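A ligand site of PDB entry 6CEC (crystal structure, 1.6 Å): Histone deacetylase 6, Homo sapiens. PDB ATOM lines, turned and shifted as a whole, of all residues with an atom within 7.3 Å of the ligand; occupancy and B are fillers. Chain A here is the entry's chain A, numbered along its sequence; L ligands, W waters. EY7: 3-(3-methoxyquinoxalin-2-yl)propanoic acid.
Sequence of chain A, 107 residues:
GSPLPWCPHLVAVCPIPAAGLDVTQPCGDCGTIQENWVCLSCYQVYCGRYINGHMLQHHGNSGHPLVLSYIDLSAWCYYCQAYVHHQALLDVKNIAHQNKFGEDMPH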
ATOM      1  N   GLU A  35      -3.593  24.009 -31.424  1.00  0.00           N
ATOM      2  CA  GLU A  35      -3.169  24.195 -30.049  1.00  0.00           C
ATOM      3  C   GLU A  35      -3.076  22.888 -29.271  1.00  0.00           C
ATOM      4  O   GLU A  35      -3.473  22.826 -28.103  1.00  0.00           O
ATOM      5  CB  GLU A  35      -4.142  25.122 -29.302  1.00  0.00           C
ATOM      6  CG  GLU A  35      -4.351  26.455 -29.949  1.00  0.00           C
ATOM      7  CD  GLU A  35      -3.502  27.529 -29.318  1.00  0.00           C
ATOM      8  OE1 GLU A  35      -3.529  27.630 -28.066  1.00  0.00           O
ATOM      9  OE2 GLU A  35      -2.891  28.294 -30.088  1.00  0.00           O
ATOM     10  N   TRP A  37      -1.156  19.824 -27.220  1.00  0.00           N
ATOM     11  CA  TRP A  37      -0.145  19.561 -26.191  1.00  0.00           C
ATOM     12  C   TRP A  37       0.045  18.056 -26.092  1.00  0.00           C
ATOM     13  O   TRP A  37      -0.858  17.282 -26.431  1.00  0.00           O
ATOM     14  CB  TRP A  37      -0.595  20.078 -24.838  1.00  0.00           C
ATOM     15  CG  TRP A  37      -0.833  21.531 -24.737  1.00  0.00           C
ATOM     16  CD1 TRP A  37      -1.860  22.240 -25.291  1.00  0.00           C
ATOM     17  CD2 TRP A  37      -0.019  22.493 -24.036  1.00  0.00           C
ATOM     18  NE1 TRP A  37      -1.740  23.571 -24.979  1.00  0.00           N
ATOM     19  CE2 TRP A  37      -0.634  23.748 -24.197  1.00  0.00           C
ATOM     20  CE3 TRP A  37       1.159  22.436 -23.268  1.00  0.00           C
ATOM     21  CZ2 TRP A  37      -0.122  24.911 -23.612  1.00  0.00           C
ATOM     22  CZ3 TRP A  37       1.636  23.582 -22.673  1.00  0.00           C
ATOM     23  CH2 TRP A  37       1.019  24.790 -22.853  1.00  0.00           C
ATOM     24  N   TYR A  46      -3.591  16.084 -26.707  1.00  0.00           N
ATOM     25  CA  TYR A  46      -4.936  16.641 -26.549  1.00  0.00           C
ATOM     26  C   TYR A  46      -4.839  18.157 -26.680  1.00  0.00           C
ATOM     27  O   TYR A  46      -3.784  18.745 -26.432  1.00  0.00           O
ATOM     28  CB  TYR A  46      -5.549  16.283 -25.196  1.00  0.00           C
ATOM     29  CG  TYR A  46      -5.818  14.812 -24.946  1.00  0.00           C
ATOM     30  CD1 TYR A  46      -6.812  14.145 -25.639  1.00  0.00           C
ATOM     31  CD2 TYR A  46      -5.053  14.107 -24.023  1.00  0.00           C
ATOM     32  CE1 TYR A  46      -7.061  12.821 -25.405  1.00  0.00           C
ATOM     33  CE2 TYR A  46      -5.275  12.722 -23.819  1.00  0.00           C
ATOM     34  CZ  TYR A  46      -6.283  12.119 -24.522  1.00  0.00           C
ATOM     35  OH  TYR A  46      -6.527  10.764 -24.320  1.00  0.00           O
ATOM     36  N   CYS A  47      -5.971  18.765 -27.019  1.00  0.00           N
ATOM     37  CA  CYS A  47      -5.990  20.202 -27.288  1.00  0.00           C
ATOM     38  C   CYS A  47      -6.006  21.102 -26.082  1.00  0.00           C
ATOM     39  O   CYS A  47      -6.398  20.732 -24.979  1.00  0.00           O
ATOM     40  CB  CYS A  47      -7.136  20.564 -28.237  1.00  0.00           C
ATOM     41  SG  CYS A  47      -8.792  20.331 -27.549  1.00  0.00           S
ATOM     42  N   GLY A  48      -5.538  22.308 -26.346  1.00  0.00           N
ATOM     43  CA  GLY A  48      -5.473  23.345 -25.322  1.00  0.00           C
ATOM     44  C   GLY A  48      -6.785  23.976 -24.889  1.00  0.00           C
ATOM     45  O   GLY A  48      -7.838  23.805 -25.508  1.00  0.00           O
ATOM     46  N   ARG A  49      -6.682  24.783 -23.818  1.00  0.00           N
ATOM     47  CA  ARG A  49      -7.857  25.389 -23.198  1.00  0.00           C
ATOM     48  C   ARG A  49      -8.659  26.304 -24.121  1.00  0.00           C
ATOM     49  O   ARG A  49      -9.882  26.378 -24.000  1.00  0.00           O
ATOM     50  CB  ARG A  49      -7.431  26.178 -21.903  1.00  0.00           C
ATOM     51  CG  ARG A  49      -6.609  27.438 -22.129  1.00  0.00           C
ATOM     52  CD  ARG A  49      -5.699  27.842 -20.934  1.00  0.00           C
ATOM     53  NE  ARG A  49      -4.761  28.935 -21.226  1.00  0.00           N
ATOM     54  CZ  ARG A  49      -3.640  28.865 -21.972  1.00  0.00           C
ATOM     55  NH1 ARG A  49      -2.862  29.931 -22.162  1.00  0.00           N
ATOM     56  NH2 ARG A  49      -3.272  27.735 -22.556  1.00  0.00           N
ATOM     57  N   TYR A  50      -8.008  26.933 -25.090  1.00  0.00           N
ATOM     58  CA  TYR A  50      -8.722  27.817 -26.043  1.00  0.00           C
ATOM     59  C   TYR A  50      -9.411  27.129 -27.191  1.00  0.00           C
ATOM     60  O   TYR A  50     -10.141  27.775 -27.946  1.00  0.00           O
ATOM     61  CB  TYR A  50      -7.773  28.904 -26.531  1.00  0.00           C
ATOM     62  CG  TYR A  50      -7.296  29.840 -25.399  1.00  0.00           C
ATOM     63  CD1 TYR A  50      -8.239  30.445 -24.544  1.00  0.00           C
ATOM     64  CD2 TYR A  50      -5.964  30.042 -25.111  1.00  0.00           C
ATOM     65  CE1 TYR A  50      -7.827  31.313 -23.503  1.00  0.00           C
ATOM     66  CE2 TYR A  50      -5.542  30.897 -24.097  1.00  0.00           C
ATOM     67  CZ  TYR A  50      -6.494  31.508 -23.251  1.00  0.00           C
ATOM     68  OH  TYR A  50      -6.146  32.367 -22.204  1.00  0.00           O
ATOM     69  N   ILE A  51      -9.204  25.815 -27.363  1.00  0.00           N
ATOM     70  CA  ILE A  51      -9.923  25.022 -28.330  1.00  0.00           C
ATOM     71  C   ILE A  51     -11.003  24.287 -27.574  1.00  0.00           C
ATOM     72  O   ILE A  51     -12.050  24.905 -27.286  1.00  0.00           O
ATOM     73  CB  ILE A  51      -8.972  24.110 -29.151  1.00  0.00           C
ATOM     74  CG1 ILE A  51      -7.764  24.883 -29.652  1.00  0.00           C
ATOM     75  CG2 ILE A  51      -9.799  23.420 -30.270  1.00  0.00           C
ATOM     76  CD1 ILE A  51      -8.099  26.016 -30.616  1.00  0.00           C
ATOM     77  N   GLY A  53     -10.265  22.171 -24.684  1.00  0.00           N
ATOM     78  CA  GLY A  53      -9.781  21.878 -23.345  1.00  0.00           C
ATOM     79  C   GLY A  53      -9.604  20.426 -23.000  1.00  0.00           C
ATOM     80  O   GLY A  53      -9.733  20.011 -21.836  1.00  0.00           O
ATOM     81  N   HIS A  54      -9.281  19.605 -23.992  1.00  0.00           N
ATOM     82  CA  HIS A  54      -9.118  18.192 -23.754  1.00  0.00           C
ATOM     83  C   HIS A  54      -7.883  17.852 -22.955  1.00  0.00           C
ATOM     84  O   HIS A  54      -7.948  16.880 -22.193  1.00  0.00           O
ATOM     85  CB  HIS A  54      -9.253  17.402 -25.053  1.00  0.00           C
ATOM     86  CG  HIS A  54     -10.650  17.444 -25.561  1.00  0.00           C
ATOM     87  ND1 HIS A  54     -10.996  17.799 -26.863  1.00  0.00           N
ATOM     88  CD2 HIS A  54     -11.817  17.209 -24.908  1.00  0.00           C
ATOM     89  CE1 HIS A  54     -12.318  17.759 -26.965  1.00  0.00           C
ATOM     90  NE2 HIS A  54     -12.835  17.404 -25.802  1.00  0.00           N
ATOM     91  N   MET A  55      -6.813  18.639 -23.050  1.00  0.00           N
ATOM     92  CA  MET A  55      -5.657  18.334 -22.187  1.00  0.00           C
ATOM     93  C   MET A  55      -5.964  18.638 -20.730  1.00  0.00           C
ATOM     94  O   MET A  55      -5.577  17.872 -19.842  1.00  0.00           O
ATOM     95  CB  MET A  55      -4.338  18.992 -22.637  1.00  0.00           C
ATOM     96  CG  MET A  55      -3.098  18.514 -21.859  1.00  0.00           C
ATOM     97  SD  MET A  55      -2.864  16.718 -22.040  1.00  0.00           S
ATOM     98  CE  MET A  55      -1.951  16.642 -23.564  1.00  0.00           C
ATOM     99  N   LEU A  56      -6.716  19.727 -20.457  1.00  0.00           N
ATOM    100  CA  LEU A  56      -7.136  20.014 -19.102  1.00  0.00           C
ATOM    101  C   LEU A  56      -8.036  18.888 -18.577  1.00  0.00           C
ATOM    102  O   LEU A  56      -7.865  18.421 -17.436  1.00  0.00           O
ATOM    103  CB  LEU A  56      -7.823  21.405 -19.048  1.00  0.00           C
ATOM    104  CG  LEU A  56      -8.332  21.859 -17.698  1.00  0.00           C
ATOM    105  CD1 LEU A  56      -7.290  21.985 -16.632  1.00  0.00           C
ATOM    106  CD2 LEU A  56      -9.022  23.205 -17.924  1.00  0.00           C
ATOM    107  N   GLN A  57      -8.942  18.360 -19.407  1.00  0.00           N
ATOM    108  CA  GLN A  57      -9.754  17.257 -19.010  1.00  0.00           C
ATOM    109  C   GLN A  57      -8.905  16.018 -18.705  1.00  0.00           C
ATOM    110  O   GLN A  57      -9.135  15.298 -17.710  1.00  0.00           O
ATOM    111  CB  GLN A  57     -10.801  16.951 -20.093  1.00  0.00           C
ATOM    112  CG  GLN A  57     -11.733  15.798 -19.823  1.00  0.00           C
ATOM    113  CD  GLN A  57     -12.785  15.658 -20.929  1.00  0.00           C
ATOM    114  OE1 GLN A  57     -12.962  16.572 -21.734  1.00  0.00           O
ATOM    115  NE2 GLN A  57     -13.465  14.513 -20.972  1.00  0.00           N
ATOM    116  N   VAL A  67       2.707  19.058 -19.273  1.00  0.00           N
ATOM    117  CA  VAL A  67       2.325  18.942 -20.678  1.00  0.00           C
ATOM    118  C   VAL A  67       3.184  19.918 -21.507  1.00  0.00           C
ATOM    119  O   VAL A  67       3.546  20.995 -21.025  1.00  0.00           O
ATOM    120  CB  VAL A  67       0.784  19.153 -20.851  1.00  0.00           C
ATOM    121  CG1 VAL A  67      -0.012  18.078 -20.114  1.00  0.00           C
ATOM    122  CG2 VAL A  67       0.293  20.516 -20.427  1.00  0.00           C
ATOM    123  N   SER A  74       6.929  25.152 -24.842  1.00  0.00           N
ATOM    124  CA  SER A  74       6.878  25.397 -23.418  1.00  0.00           C
ATOM    125  C   SER A  74       6.199  24.209 -22.716  1.00  0.00           C
ATOM    126  O   SER A  74       5.373  23.505 -23.286  1.00  0.00           O
ATOM    127  CB  SER A  74       6.090  26.629 -23.118  1.00  0.00           C
ATOM    128  OG  SER A  74       4.777  26.536 -23.566  1.00  0.00           O
ATOM    129  N   TRP A  76       3.958  23.231 -19.278  1.00  0.00           N
ATOM    130  CA  TRP A  76       3.049  23.730 -18.273  1.00  0.00           C
ATOM    131  C   TRP A  76       2.798  22.675 -17.238  1.00  0.00           C
ATOM    132  O   TRP A  76       2.547  21.508 -17.573  1.00  0.00           O
ATOM    133  CB  TRP A  76       1.691  24.158 -18.895  1.00  0.00           C
ATOM    134  CG  TRP A  76       0.665  24.702 -17.980  1.00  0.00           C
ATOM    135  CD1 TRP A  76      -0.446  24.055 -17.490  1.00  0.00           C
ATOM    136  CD2 TRP A  76       0.646  26.012 -17.386  1.00  0.00           C
ATOM    137  NE1 TRP A  76      -1.163  24.875 -16.664  1.00  0.00           N
ATOM    138  CE2 TRP A  76      -0.547  26.095 -16.603  1.00  0.00           C
ATOM    139  CE3 TRP A  76       1.470  27.154 -17.494  1.00  0.00           C
ATOM    140  CZ2 TRP A  76      -0.893  27.267 -15.869  1.00  0.00           C
ATOM    141  CZ3 TRP A  76       1.100  28.308 -16.782  1.00  0.00           C
ATOM    142  CH2 TRP A  76      -0.064  28.346 -15.990  1.00  0.00           C
ATOM    143  N   CYS A  77       2.846  23.060 -15.960  1.00  0.00           N
ATOM    144  CA  CYS A  77       2.415  22.197 -14.882  1.00  0.00           C
ATOM    145  C   CYS A  77       1.056  22.626 -14.395  1.00  0.00           C
ATOM    146  O   CYS A  77       0.902  23.720 -13.897  1.00  0.00           O
ATOM    147  CB  CYS A  77       3.373  22.195 -13.706  1.00  0.00           C
ATOM    148  SG  CYS A  77       2.847  21.078 -12.373  1.00  0.00           S
ATOM    149  N   TYR A  78       0.100  21.728 -14.443  1.00  0.00           N
ATOM    150  CA  TYR A  78      -1.275  22.082 -14.032  1.00  0.00           C
ATOM    151  C   TYR A  78      -1.414  22.255 -12.521  1.00  0.00           C
ATOM    152  O   TYR A  78      -2.344  22.922 -12.074  1.00  0.00           O
ATOM    153  CB  TYR A  78      -2.288  21.024 -14.478  1.00  0.00           C
ATOM    154  CG  TYR A  78      -2.603  21.024 -15.957  1.00  0.00           C
ATOM    155  CD1 TYR A  78      -3.419  22.007 -16.541  1.00  0.00           C
ATOM    156  CD2 TYR A  78      -2.110  20.022 -16.806  1.00  0.00           C
ATOM    157  CE1 TYR A  78      -3.695  22.022 -17.920  1.00  0.00           C
ATOM    158  CE2 TYR A  78      -2.356  20.034 -18.170  1.00  0.00           C
ATOM    159  CZ  TYR A  78      -3.166  21.013 -18.722  1.00  0.00           C
ATOM    160  OH  TYR A  78      -3.421  21.002 -20.053  1.00  0.00           O
ATOM    161  N   GLN A  81       0.537  25.529 -11.733  1.00  0.00           N
ATOM    162  CA  GLN A  81      -0.092  26.609 -12.541  1.00  0.00           C
ATOM    163  C   GLN A  81       0.978  27.575 -13.001  1.00  0.00           C
ATOM    164  O   GLN A  81       0.928  28.789 -12.787  1.00  0.00           O
ATOM    165  CB  GLN A  81      -1.230  27.310 -11.801  1.00  0.00           C
ATOM    166  CG  GLN A  81      -2.244  26.349 -11.231  1.00  0.00           C
ATOM    167  CD  GLN A  81      -3.528  27.048 -10.790  1.00  0.00           C
ATOM    168  OE1 GLN A  81      -3.769  27.222  -9.611  1.00  0.00           O
ATOM    169  NE2 GLN A  81      -4.344  27.438 -11.757  1.00  0.00           N
ATOM    170  N   ALA A  82       1.991  26.987 -13.598  1.00  0.00           N
ATOM    171  CA  ALA A  82       3.176  27.680 -14.080  1.00  0.00           C
ATOM    172  C   ALA A  82       3.870  26.929 -15.209  1.00  0.00           C
ATOM    173  O   ALA A  82       3.809  25.687 -15.269  1.00  0.00           O
ATOM    174  CB  ALA A  82       4.202  27.878 -12.967  1.00  0.00           C
ATOM    175  N   TYR A  83       4.616  27.677 -16.039  1.00  0.00           N
ATOM    176  CA  TYR A  83       5.578  27.098 -16.914  1.00  0.00           C
ATOM    177  C   TYR A  83       6.813  26.670 -16.171  1.00  0.00           C
ATOM    178  O   TYR A  83       7.247  27.328 -15.198  1.00  0.00           O
ATOM    179  CB  TYR A  83       5.937  28.077 -18.014  1.00  0.00           C
ATOM    180  CG  TYR A  83       4.840  28.345 -18.980  1.00  0.00           C
ATOM    181  CD1 TYR A  83       4.497  27.407 -19.949  1.00  0.00           C
ATOM    182  CD2 TYR A  83       4.183  29.531 -18.957  1.00  0.00           C
ATOM    183  CE1 TYR A  83       3.499  27.674 -20.865  1.00  0.00           C
ATOM    184  CE2 TYR A  83       3.147  29.777 -19.856  1.00  0.00           C
ATOM    185  CZ  TYR A  83       2.846  28.848 -20.792  1.00  0.00           C
ATOM    186  OH  TYR A  83       1.839  29.118 -21.709  1.00  0.00           O
HETATM  187  O1  EY7 L   1      -4.196  24.940 -22.337  1.00  0.00           O
HETATM  188  O2  EY7 L   1      -4.583  23.011 -21.243  1.00  0.00           O
HETATM  189  C3  EY7 L   1      -1.902  25.321 -20.672  1.00  0.00           C
HETATM  190  C5  EY7 L   1      -3.852  23.914 -21.547  1.00  0.00           C
HETATM  191  C7  EY7 L   1      -5.527  25.612 -17.490  1.00  0.00           C
HETATM  192  C8  EY7 L   1      -6.237  26.299 -16.540  1.00  0.00           C
HETATM  193  C9  EY7 L   1      -5.869  27.597 -16.188  1.00  0.00           C
HETATM  194  C4  EY7 L   1      -2.446  23.945 -21.031  1.00  0.00           C
HETATM  195  C2  EY7 L   1      -2.683  26.075 -19.633  1.00  0.00           C
HETATM  196  N   EY7 L   1      -3.718  25.497 -19.059  1.00  0.00           N
HETATM  197  C6  EY7 L   1      -4.411  26.206 -18.120  1.00  0.00           C
HETATM  198  C11 EY7 L   1      -4.029  27.520 -17.759  1.00  0.00           C
HETATM  199  C10 EY7 L   1      -4.793  28.205 -16.776  1.00  0.00           C
HETATM  200  N1  EY7 L   1      -2.941  28.140 -18.329  1.00  0.00           N
HETATM  201  C1  EY7 L   1      -2.300  27.444 -19.218  1.00  0.00           C
HETATM  202  O   EY7 L   1      -1.180  27.860 -19.851  1.00  0.00           O
HETATM  203  C   EY7 L   1      -0.815  29.248 -19.704  1.00  0.00           C
HETATM  204  O   HOH W   1      -6.784  21.879 -22.380  1.00  0.00           O
HETATM  205  O   HOH W   2      -2.705  30.822 -17.101  1.00  0.00           O
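Residues that only touch the ligand: Trp 37 (3.5 Å), Gly 48 (3.6 Å), Leu 56 (3.99 Å), Trp 76 (3.3 Å) and Tyr 83 (3.3 Å). Hydrophobic or aromatic side chains within 4 Å of the ligand: Trp 37, Trp 76, Tyr 78 and Tyr 83. The nearest printed residue that does not touch the ligand is Met 55 (4.3 Å).
The backbone NH (N) of Trp 76 sits at hydrogen-bond distance from the backbone carbonyl oxygen (O) of Val 67 (2.9 Å). O of Tyr 46 sits at hydrogen-bond distance from N of Trp 37 (2.9 Å). The backbone NH (N) of Gly 53 sits at hydrogen-bond distance from the backbone carbonyl oxygen (O) of Gly 48, 3.0 Å away. The backbone NH (N) of Gly 48 sits at hydrogen-bond distance from the backbone carbonyl oxygen (O) of Glu 35.
OH of Tyr 78 sits at hydrogen-bond distance from O2 of the ligand (2.6 Å). An oxygen (O1) of the ligand sits at hydrogen-bond distance from the backbone NH (N) of Arg 49. NH2 of Arg 49 is in salt-bridge range of O1 of the ligand.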
